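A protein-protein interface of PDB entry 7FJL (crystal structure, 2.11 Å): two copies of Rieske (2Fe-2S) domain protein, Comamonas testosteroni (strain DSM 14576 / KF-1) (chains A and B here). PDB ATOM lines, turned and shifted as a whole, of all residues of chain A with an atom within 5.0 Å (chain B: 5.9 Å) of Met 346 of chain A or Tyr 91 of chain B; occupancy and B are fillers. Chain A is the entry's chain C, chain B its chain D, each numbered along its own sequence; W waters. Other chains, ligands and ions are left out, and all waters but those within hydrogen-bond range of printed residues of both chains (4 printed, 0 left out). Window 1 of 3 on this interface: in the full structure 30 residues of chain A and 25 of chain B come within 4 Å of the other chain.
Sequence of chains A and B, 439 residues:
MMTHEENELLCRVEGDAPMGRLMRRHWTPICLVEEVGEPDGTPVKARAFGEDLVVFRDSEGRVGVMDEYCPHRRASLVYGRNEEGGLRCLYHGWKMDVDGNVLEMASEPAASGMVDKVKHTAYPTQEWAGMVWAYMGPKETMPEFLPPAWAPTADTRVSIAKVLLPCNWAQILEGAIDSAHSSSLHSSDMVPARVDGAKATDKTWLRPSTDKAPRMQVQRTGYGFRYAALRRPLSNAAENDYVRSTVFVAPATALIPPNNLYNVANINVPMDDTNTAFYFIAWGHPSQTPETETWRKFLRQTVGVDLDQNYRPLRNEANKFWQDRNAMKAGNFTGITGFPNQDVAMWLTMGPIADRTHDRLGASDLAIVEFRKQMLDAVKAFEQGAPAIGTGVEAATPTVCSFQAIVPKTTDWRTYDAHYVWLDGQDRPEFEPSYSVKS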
ATOM      1  N   GLY A 175      -5.115  -6.074  -9.875  1.00  0.00           N
ATOM      2  CA  GLY A 175      -5.554  -5.715 -11.221  1.00  0.00           C
ATOM      3  C   GLY A 175      -5.545  -4.183 -11.455  1.00  0.00           C
ATOM      4  O   GLY A 175      -5.374  -3.741 -12.581  1.00  0.00           O
ATOM      5  N   ASP A 178      -1.404  -2.797 -12.557  1.00  0.00           N
ATOM      6  CA  ASP A 178      -0.975  -3.775 -13.543  1.00  0.00           C
ATOM      7  C   ASP A 178      -1.078  -3.154 -14.940  1.00  0.00           C
ATOM      8  O   ASP A 178      -1.727  -3.683 -15.855  1.00  0.00           O
ATOM      9  CB  ASP A 178      -1.816  -5.034 -13.338  1.00  0.00           C
ATOM     10  CG  ASP A 178      -1.439  -6.211 -14.217  1.00  0.00           C
ATOM     11  OD1 ASP A 178      -0.320  -6.186 -14.793  1.00  0.00           O
ATOM     12  OD2 ASP A 178      -2.275  -7.204 -14.276  1.00  0.00           O
ATOM     13  N   HIS A 181      -1.748  -4.694 -18.418  1.00  0.00           N
ATOM     14  CA  HIS A 181      -2.990  -5.369 -18.815  1.00  0.00           C
ATOM     15  C   HIS A 181      -3.882  -4.531 -19.752  1.00  0.00           C
ATOM     16  O   HIS A 181      -4.582  -5.084 -20.597  1.00  0.00           O
ATOM     17  CB  HIS A 181      -3.742  -5.918 -17.612  1.00  0.00           C
ATOM     18  CG  HIS A 181      -4.721  -4.931 -17.063  1.00  0.00           C
ATOM     19  ND1 HIS A 181      -4.338  -3.847 -16.332  1.00  0.00           N
ATOM     20  CD2 HIS A 181      -6.066  -4.867 -17.161  1.00  0.00           C
ATOM     21  CE1 HIS A 181      -5.395  -3.155 -15.971  1.00  0.00           C
ATOM     22  NE2 HIS A 181      -6.466  -3.764 -16.454  1.00  0.00           N
ATOM     23  N   SER A 184      -3.512  -5.399 -23.411  1.00  0.00           N
ATOM     24  CA  SER A 184      -4.175  -6.578 -23.956  1.00  0.00           C
ATOM     25  C   SER A 184      -5.684  -6.475 -23.740  1.00  0.00           C
ATOM     26  O   SER A 184      -6.454  -6.115 -24.656  1.00  0.00           O
ATOM     27  CB  SER A 184      -3.647  -7.863 -23.349  1.00  0.00           C
ATOM     28  OG  SER A 184      -2.311  -8.056 -23.777  1.00  0.00           O
ATOM     29  N   LEU A 185      -6.079  -6.796 -22.490  1.00  0.00           N
ATOM     30  CA  LEU A 185      -7.460  -6.903 -22.074  1.00  0.00           C
ATOM     31  C   LEU A 185      -8.267  -5.688 -22.557  1.00  0.00           C
ATOM     32  O   LEU A 185      -9.392  -5.840 -23.065  1.00  0.00           O
ATOM     33  CB  LEU A 185      -7.499  -7.063 -20.560  1.00  0.00           C
ATOM     34  CG  LEU A 185      -8.864  -7.420 -19.982  1.00  0.00           C
ATOM     35  CD1 LEU A 185      -9.249  -8.853 -20.338  1.00  0.00           C
ATOM     36  CD2 LEU A 185      -8.892  -7.166 -18.466  1.00  0.00           C
ATOM     37  N   GLN A 342     -14.356  -6.795 -18.075  1.00  0.00           N
ATOM     38  CA  GLN A 342     -13.263  -7.544 -18.647  1.00  0.00           C
ATOM     39  C   GLN A 342     -12.317  -7.920 -17.496  1.00  0.00           C
ATOM     40  O   GLN A 342     -11.789  -9.021 -17.489  1.00  0.00           O
ATOM     41  CB  GLN A 342     -12.608  -6.704 -19.769  1.00  0.00           C
ATOM     42  CG  GLN A 342     -13.560  -6.334 -20.946  1.00  0.00           C
ATOM     43  CD  GLN A 342     -13.044  -5.175 -21.809  1.00  0.00           C
ATOM     44  OE1 GLN A 342     -11.957  -4.599 -21.597  1.00  0.00           O
ATOM     45  NE2 GLN A 342     -13.852  -4.742 -22.772  1.00  0.00           N
ATOM     46  N   ASP A 343     -12.095  -6.978 -16.564  1.00  0.00           N
ATOM     47  CA  ASP A 343     -11.267  -7.171 -15.383  1.00  0.00           C
ATOM     48  C   ASP A 343     -11.884  -8.282 -14.534  1.00  0.00           C
ATOM     49  O   ASP A 343     -11.211  -9.232 -14.150  1.00  0.00           O
ATOM     50  CB  ASP A 343     -11.097  -5.877 -14.572  1.00  0.00           C
ATOM     51  CG  ASP A 343     -10.127  -4.871 -15.212  1.00  0.00           C
ATOM     52  OD1 ASP A 343     -10.469  -3.655 -15.286  1.00  0.00           O
ATOM     53  OD2 ASP A 343      -9.040  -5.295 -15.671  1.00  0.00           O
ATOM     54  N   VAL A 344     -13.198  -8.178 -14.293  1.00  0.00           N
ATOM     55  CA  VAL A 344     -13.868  -9.085 -13.389  1.00  0.00           C
ATOM     56  C   VAL A 344     -13.726 -10.508 -13.930  1.00  0.00           C
ATOM     57  O   VAL A 344     -13.486 -11.432 -13.147  1.00  0.00           O
ATOM     58  CB  VAL A 344     -15.325  -8.616 -13.206  1.00  0.00           C
ATOM     59  CG1 VAL A 344     -16.249  -9.680 -12.620  1.00  0.00           C
ATOM     60  CG2 VAL A 344     -15.319  -7.377 -12.334  1.00  0.00           C
ATOM     61  N   ALA A 345     -13.890 -10.711 -15.252  1.00  0.00           N
ATOM     62  CA  ALA A 345     -13.826 -12.071 -15.802  1.00  0.00           C
ATOM     63  C   ALA A 345     -12.481 -12.692 -15.455  1.00  0.00           C
ATOM     64  O   ALA A 345     -12.404 -13.884 -15.214  1.00  0.00           O
ATOM     65  CB  ALA A 345     -14.032 -12.108 -17.307  1.00  0.00           C
ATOM     66  N   MET A 346     -11.415 -11.876 -15.466  1.00  0.00           N
ATOM     67  CA  MET A 346     -10.079 -12.402 -15.211  1.00  0.00           C
ATOM     68  C   MET A 346      -9.936 -12.754 -13.716  1.00  0.00           C
ATOM     69  O   MET A 346      -9.610 -13.896 -13.389  1.00  0.00           O
ATOM     70  CB  MET A 346      -8.945 -11.461 -15.660  1.00  0.00           C
ATOM     71  CG  MET A 346      -8.965 -11.002 -17.140  1.00  0.00           C
ATOM     72  SD  MET A 346      -8.622 -12.390 -18.292  1.00  0.00           S
ATOM     73  CE  MET A 346     -10.255 -13.133 -18.496  1.00  0.00           C
ATOM     74  N   TRP A 347     -10.284 -11.825 -12.819  1.00  0.00           N
ATOM     75  CA  TRP A 347     -10.184 -11.994 -11.369  1.00  0.00           C
ATOM     76  C   TRP A 347     -10.990 -13.200 -10.874  1.00  0.00           C
ATOM     77  O   TRP A 347     -10.447 -13.979 -10.086  1.00  0.00           O
ATOM     78  CB  TRP A 347     -10.668 -10.711 -10.652  1.00  0.00           C
ATOM     79  CG  TRP A 347      -9.928  -9.471 -11.075  1.00  0.00           C
ATOM     80  CD1 TRP A 347      -8.640  -9.373 -11.564  1.00  0.00           C
ATOM     81  CD2 TRP A 347     -10.441  -8.127 -11.008  1.00  0.00           C
ATOM     82  NE1 TRP A 347      -8.323  -8.048 -11.805  1.00  0.00           N
ATOM     83  CE2 TRP A 347      -9.409  -7.262 -11.467  1.00  0.00           C
ATOM     84  CE3 TRP A 347     -11.642  -7.566 -10.572  1.00  0.00           C
ATOM     85  CZ2 TRP A 347      -9.583  -5.869 -11.507  1.00  0.00           C
ATOM     86  CZ3 TRP A 347     -11.806  -6.189 -10.593  1.00  0.00           C
ATOM     87  CH2 TRP A 347     -10.791  -5.356 -11.071  1.00  0.00           C
ATOM     88  N   LEU A 348     -12.275 -13.323 -11.296  1.00  0.00           N
ATOM     89  CA  LEU A 348     -13.126 -14.366 -10.737  1.00  0.00           C
ATOM     90  C   LEU A 348     -12.667 -15.718 -11.258  1.00  0.00           C
ATOM     91  O   LEU A 348     -12.797 -16.692 -10.529  1.00  0.00           O
ATOM     92  CB  LEU A 348     -14.615 -14.159 -11.079  1.00  0.00           C
ATOM     93  CG  LEU A 348     -15.165 -12.823 -10.604  1.00  0.00           C
ATOM     94  CD1 LEU A 348     -16.726 -12.835 -10.707  1.00  0.00           C
ATOM     95  CD2 LEU A 348     -14.685 -12.586  -9.165  1.00  0.00           C
ATOM     96  N   THR A 349     -12.097 -15.773 -12.459  1.00  0.00           N
ATOM     97  CA  THR A 349     -11.673 -17.087 -12.929  1.00  0.00           C
ATOM     98  C   THR A 349     -10.360 -17.578 -12.306  1.00  0.00           C
ATOM     99  O   THR A 349     -10.010 -18.737 -12.494  1.00  0.00           O
ATOM    100  CB  THR A 349     -11.649 -17.200 -14.452  1.00  0.00           C
ATOM    101  OG1 THR A 349     -10.572 -16.466 -15.042  1.00  0.00           O
ATOM    102  CG2 THR A 349     -13.015 -16.941 -15.046  1.00  0.00           C
ATOM    103  N   MET A 350      -9.662 -16.703 -11.563  1.00  0.00           N
ATOM    104  CA  MET A 350      -8.565 -17.128 -10.716  1.00  0.00           C
ATOM    105  C   MET A 350      -9.017 -17.891  -9.470  1.00  0.00           C
ATOM    106  O   MET A 350      -8.150 -18.422  -8.755  1.00  0.00           O
ATOM    107  CB  MET A 350      -7.741 -15.914 -10.285  1.00  0.00           C
ATOM    108  CG  MET A 350      -7.061 -15.267 -11.445  1.00  0.00           C
ATOM    109  SD  MET A 350      -6.485 -13.699 -10.781  1.00  0.00           S
ATOM    110  CE  MET A 350      -5.797 -13.075 -12.305  1.00  0.00           C
ATOM    111  N   HIS B  72       0.555 -17.559 -16.480  1.00  0.00           N
ATOM    112  CA  HIS B  72       0.919 -16.268 -15.898  1.00  0.00           C
ATOM    113  C   HIS B  72       0.284 -16.018 -14.517  1.00  0.00           C
ATOM    114  O   HIS B  72       0.963 -16.198 -13.500  1.00  0.00           O
ATOM    115  CB  HIS B  72       0.634 -15.130 -16.889  1.00  0.00           C
ATOM    116  CG  HIS B  72       1.020 -13.793 -16.372  1.00  0.00           C
ATOM    117  ND1 HIS B  72       0.322 -12.649 -16.726  1.00  0.00           N
ATOM    118  CD2 HIS B  72       2.023 -13.393 -15.526  1.00  0.00           C
ATOM    119  CE1 HIS B  72       0.874 -11.590 -16.157  1.00  0.00           C
ATOM    120  NE2 HIS B  72       1.927 -12.009 -15.390  1.00  0.00           N
ATOM    121  N   ARG B  73      -0.979 -15.541 -14.460  1.00  0.00           N
ATOM    122  CA  ARG B  73      -1.675 -15.374 -13.190  1.00  0.00           C
ATOM    123  C   ARG B  73      -3.000 -16.176 -13.097  1.00  0.00           C
ATOM    124  O   ARG B  73      -3.872 -15.852 -12.256  1.00  0.00           O
ATOM    125  CB  ARG B  73      -1.841 -13.884 -12.864  1.00  0.00           C
ATOM    126  CG  ARG B  73      -0.550 -13.060 -12.811  1.00  0.00           C
ATOM    127  CD  ARG B  73      -0.642 -12.103 -11.605  1.00  0.00           C
ATOM    128  NE  ARG B  73      -1.692 -11.079 -11.596  1.00  0.00           N
ATOM    129  CZ  ARG B  73      -1.765  -9.989 -12.368  1.00  0.00           C
ATOM    130  NH1 ARG B  73      -0.808  -9.673 -13.226  1.00  0.00           N
ATOM    131  NH2 ARG B  73      -2.814  -9.184 -12.262  1.00  0.00           N
ATOM    132  N   ARG B  74      -3.171 -17.201 -13.958  1.00  0.00           N
ATOM    133  CA  ARG B  74      -4.215 -18.195 -13.784  1.00  0.00           C
ATOM    134  C   ARG B  74      -5.655 -17.718 -14.016  1.00  0.00           C
ATOM    135  O   ARG B  74      -6.587 -18.358 -13.519  1.00  0.00           O
ATOM    136  CB  ARG B  74      -4.085 -18.909 -12.439  1.00  0.00           C
ATOM    137  CG  ARG B  74      -2.638 -19.218 -12.124  1.00  0.00           C
ATOM    138  CD  ARG B  74      -2.641 -20.231 -11.002  1.00  0.00           C
ATOM    139  NE  ARG B  74      -2.971 -21.582 -11.430  1.00  0.00           N
ATOM    140  CZ  ARG B  74      -3.954 -22.304 -10.908  1.00  0.00           C
ATOM    141  NH1 ARG B  74      -4.700 -21.817  -9.908  1.00  0.00           N
ATOM    142  NH2 ARG B  74      -4.132 -23.533 -11.380  1.00  0.00           N
ATOM    143  N   ALA B  75      -5.850 -16.650 -14.808  1.00  0.00           N
ATOM    144  CA  ALA B  75      -7.102 -16.378 -15.502  1.00  0.00           C
ATOM    145  C   ALA B  75      -7.499 -17.581 -16.374  1.00  0.00           C
ATOM    146  O   ALA B  75      -6.641 -18.309 -16.868  1.00  0.00           O
ATOM    147  CB  ALA B  75      -6.818 -15.159 -16.382  1.00  0.00           C
ATOM    148  N   SER B  76      -8.806 -17.728 -16.684  1.00  0.00           N
ATOM    149  CA  SER B  76      -9.213 -18.893 -17.436  1.00  0.00           C
ATOM    150  C   SER B  76      -8.936 -18.671 -18.919  1.00  0.00           C
ATOM    151  O   SER B  76      -9.365 -17.665 -19.490  1.00  0.00           O
ATOM    152  CB  SER B  76     -10.666 -19.173 -17.242  1.00  0.00           C
ATOM    153  OG  SER B  76     -11.047 -20.127 -18.212  1.00  0.00           O
ATOM    154  N   TYR B  79     -11.628 -18.139 -21.911  1.00  0.00           N
ATOM    155  CA  TYR B  79     -12.040 -16.839 -22.451  1.00  0.00           C
ATOM    156  C   TYR B  79     -11.127 -16.315 -23.568  1.00  0.00           C
ATOM    157  O   TYR B  79     -11.396 -15.233 -24.084  1.00  0.00           O
ATOM    158  CB  TYR B  79     -12.158 -15.770 -21.351  1.00  0.00           C
ATOM    159  CG  TYR B  79     -13.233 -16.131 -20.364  1.00  0.00           C
ATOM    160  CD1 TYR B  79     -14.528 -15.642 -20.561  1.00  0.00           C
ATOM    161  CD2 TYR B  79     -12.984 -17.047 -19.326  1.00  0.00           C
ATOM    162  CE1 TYR B  79     -15.552 -16.040 -19.711  1.00  0.00           C
ATOM    163  CE2 TYR B  79     -14.009 -17.469 -18.495  1.00  0.00           C
ATOM    164  CZ  TYR B  79     -15.295 -16.987 -18.728  1.00  0.00           C
ATOM    165  OH  TYR B  79     -16.339 -17.322 -17.930  1.00  0.00           O
ATOM    166  N   CYS B  89      -4.350 -15.758 -23.849  1.00  0.00           N
ATOM    167  CA  CYS B  89      -5.032 -15.241 -22.667  1.00  0.00           C
ATOM    168  C   CYS B  89      -5.416 -13.783 -22.877  1.00  0.00           C
ATOM    169  O   CYS B  89      -4.672 -13.033 -23.494  1.00  0.00           O
ATOM    170  CB  CYS B  89      -4.138 -15.398 -21.451  1.00  0.00           C
ATOM    171  SG  CYS B  89      -4.969 -14.909 -19.922  1.00  0.00           S
ATOM    172  N   LEU B  90      -6.622 -13.391 -22.480  1.00  0.00           N
ATOM    173  CA  LEU B  90      -7.068 -12.014 -22.634  1.00  0.00           C
ATOM    174  C   LEU B  90      -6.282 -11.064 -21.735  1.00  0.00           C
ATOM    175  O   LEU B  90      -6.242  -9.878 -22.043  1.00  0.00           O
ATOM    176  CB  LEU B  90      -8.561 -11.838 -22.281  1.00  0.00           C
ATOM    177  CG  LEU B  90      -9.540 -12.698 -23.076  1.00  0.00           C
ATOM    178  CD1 LEU B  90     -10.988 -12.503 -22.592  1.00  0.00           C
ATOM    179  CD2 LEU B  90      -9.395 -12.537 -24.587  1.00  0.00           C
ATOM    180  N   TYR B  91      -5.723 -11.563 -20.611  1.00  0.00           N
ATOM    181  CA  TYR B  91      -5.311 -10.684 -19.517  1.00  0.00           C
ATOM    182  C   TYR B  91      -4.045  -9.882 -19.913  1.00  0.00           C
ATOM    183  O   TYR B  91      -4.083  -8.649 -19.947  1.00  0.00           O
ATOM    184  CB  TYR B  91      -5.177 -11.481 -18.203  1.00  0.00           C
ATOM    185  CG  TYR B  91      -5.333 -10.627 -16.952  1.00  0.00           C
ATOM    186  CD1 TYR B  91      -5.622  -9.268 -17.032  1.00  0.00           C
ATOM    187  CD2 TYR B  91      -5.245 -11.170 -15.684  1.00  0.00           C
ATOM    188  CE1 TYR B  91      -5.747  -8.471 -15.900  1.00  0.00           C
ATOM    189  CE2 TYR B  91      -5.422 -10.409 -14.542  1.00  0.00           C
ATOM    190  CZ  TYR B  91      -5.651  -9.052 -14.647  1.00  0.00           C
ATOM    191  OH  TYR B  91      -5.812  -8.310 -13.484  1.00  0.00           O
ATOM    192  N   HIS B  92      -2.941 -10.577 -20.273  1.00  0.00           N
ATOM    193  CA  HIS B  92      -1.727  -9.860 -20.673  1.00  0.00           C
ATOM    194  C   HIS B  92      -1.229 -10.409 -22.002  1.00  0.00           C
ATOM    195  O   HIS B  92      -0.089 -10.158 -22.411  1.00  0.00           O
ATOM    196  CB  HIS B  92      -0.631  -9.930 -19.585  1.00  0.00           C
ATOM    197  CG  HIS B  92      -1.136  -9.650 -18.217  1.00  0.00           C
ATOM    198  ND1 HIS B  92      -1.711 -10.662 -17.427  1.00  0.00           N
ATOM    199  CD2 HIS B  92      -1.318  -8.478 -17.549  1.00  0.00           C
ATOM    200  CE1 HIS B  92      -2.163 -10.156 -16.269  1.00  0.00           C
ATOM    201  NE2 HIS B  92      -1.917  -8.791 -16.310  1.00  0.00           N
ATOM    202  N   GLY B  93      -2.080 -11.239 -22.635  1.00  0.00           N
ATOM    203  CA  GLY B  93      -1.837 -11.688 -23.989  1.00  0.00           C
ATOM    204  C   GLY B  93      -0.695 -12.672 -24.128  1.00  0.00           C
ATOM    205  O   GLY B  93      -0.142 -12.793 -25.205  1.00  0.00           O
HETATM  206  O   HOH W   1      -6.834  -5.917 -14.158  1.00  0.00           O
HETATM  207  O   HOH W   2      -0.650  -6.810 -21.944  1.00  0.00           O
HETATM  208  O   HOH W   3      -5.330 -18.794  -8.869  1.00  0.00           O
HETATM  209  O   HOH W   4       1.259  -8.428 -15.326  1.00  0.00           O
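Among the printed residues, pairs that only touch across the chains: Gly 175 of chain A with Tyr 91 of chain B, Met 350 of chain A with Tyr 91 of chain B, Thr 349 of chain A with Ala 75 of chain B, Ser 184 of chain A with Tyr 91 of chain B, His 181 of chain A with His 92 of chain B, Ser 184 of chain A with Leu 90 of chain B, Met 346 of chain A with Tyr 91 of chain B, Thr 349 of chain A with Arg 74 of chain B, His 181 of chain A with Tyr 91 of chain B, Thr 349 of chain A with Tyr 79 of chain B, Met 350 of chain A with Arg 74 of chain B, Leu 185 of chain A with Tyr 91 of chain B, Asp 178 of chain A with Tyr 91 of chain B, Met 346 of chain A with Ala 75 of chain B and Met 350 of chain A with Ala 75 of chain B.
Hydrophobic or aromatic side chains of chain B within 4 Å of the printed part of chain A: Ala 75, Tyr 79, Leu 90, Tyr 91 and His 92. Along chain B the printed residues that touch a printed residue of chain A span positions 73 to 93. Printed residues of chain A that touch a printed residue of chain B: Gly 175, Asp 178, His 181, Ser 184, Leu 185, Met 346, Trp 347, Thr 349 and Met 350. Hydrophobic or aromatic side chains of chain A within 4 Å of the printed part of chain B: His 181, Leu 185, Met 346, Trp 347 and Met 350. Among the printed residues, Asp or Glu carboxylates within 4 Å of a Lys or Arg side-chain nitrogen of the other chain: Asp 178 of chain A with Arg 73 of chain B.
Of the printed residues of chain B, Asp 178 of chain A touches Arg 73, Tyr 91 and His 92. Gln 342 of chain A touches none of the printed residues of chain B. Met 346 of chain A touches two residues of chain B. His 72 of chain B touches none of the printed residues of chain A. Printed residues of chain A within 4 Å of Tyr 79 of chain B: Thr 349. Tyr 91 of chain B touches just these residues of chain A: Gly 175 (3.5 Å), Asp 178 (3.8 Å), His 181 (3.6 Å), Ser 184 (3.5 Å), Leu 185 (3.7 Å), Met 346 (3.6 Å), Trp 347 (3.0 Å) and Met 350 (3.5 Å). Printed residues of chain A within 4 Å of His 92 of chain B: Asp 178, His 181 and Ser 184. The nearest residue of chain B that does not touch Met 346 of chain A is Leu 90 of chain B (4.03 Å). The nearest printed residue of chain A that does not touch Tyr 79 of chain B is Met 346 of chain A (4.3 Å).
The side-chain carboxylate of Asp 178 of chain A is in salt-bridge range of the guanidinium group of Arg 73 of chain B (2.9 Å). The side-chain carboxylate (OD2) of Asp 178 of chain A lies within hydrogen-bond range of a ring nitrogen (NE2) of His 92 of chain B (2.6 Å). OG of Ser 184 of chain A sits close to O of His 92 of chain B (3.3 Å). The backbone NH (N) of Gly 93 of chain B is in hydrogen-bond range of the side-chain hydroxyl (OG) of Ser 184 of chain A (3.4 Å). The backbone NH of Leu 185 of chain A lies within hydrogen-bond range of the backbone carbonyl oxygen of Leu 90 of chain B, 3.1 Å away. The indole nitrogen (NE1) of Trp 347 of chain A sits at hydrogen-bond distance from the side-chain hydroxyl (OH) of Tyr 91 of chain B (3.0 Å). The side-chain hydroxyl of Thr 349 of chain A is in hydrogen-bond range of the backbone NH of Ser 76 of chain B, 2.7 Å away. The side-chain sulfur (SD) of Met 350 of chain A sits close to the backbone carbonyl oxygen (O) of Arg 73 of chain B (3.7 Å).
No position is printed for both chains.
Water W1 lies within hydrogen-bond range of the side-chain hydroxyl (OH) of Tyr 91 of chain B (2.7 Å) and the backbone carbonyl oxygen (O) of Gly 175 of chain A (3.1 Å). Water W2 bridges the side-chain hydroxyl (OG) of Ser 184 of chain A (2.8 Å) and the backbone carbonyl oxygen (O) of His 92 of chain B (3.4 Å). Water W4 lies within hydrogen-bond range of the side-chain carboxylate (OD1) of Asp 178 of chain A, the guanidinium group (NH1) of Arg 73 of chain B and a ring nitrogen (NE2) of His 92 of chain B. Water W3 lies within hydrogen-bond range of O of Met 350 of chain A (2.8 Å) and NH1 of Arg 74 of chain B (3.3 Å).
ND1 of His 181 of chain A lies within hydrogen-bond range of O of Asp 178 of chain A. The side-chain amide oxygen (OE1) of Gln 342 of chain A sits close to the backbone carbonyl oxygen (O) of Leu 185 of chain A, at 3.2 Å. The backbone carbonyl oxygen (O) of Met 346 of chain A is in hydrogen-bond range of the side-chain hydroxyl (OG1) of Thr 349 of chain A, at 3.2 Å. NH2 of Arg 73 of chain B is in hydrogen-bond range of OH of Tyr 91 of chain B. NE2 of His 92 of chain B sits close to NH1 of Arg 73 of chain B (3.4 Å). The side-chain sulfur (SG) of Cys 89 of chain B lies close to the backbone NH (N) of Tyr 91 of chain B (3.5 Å).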
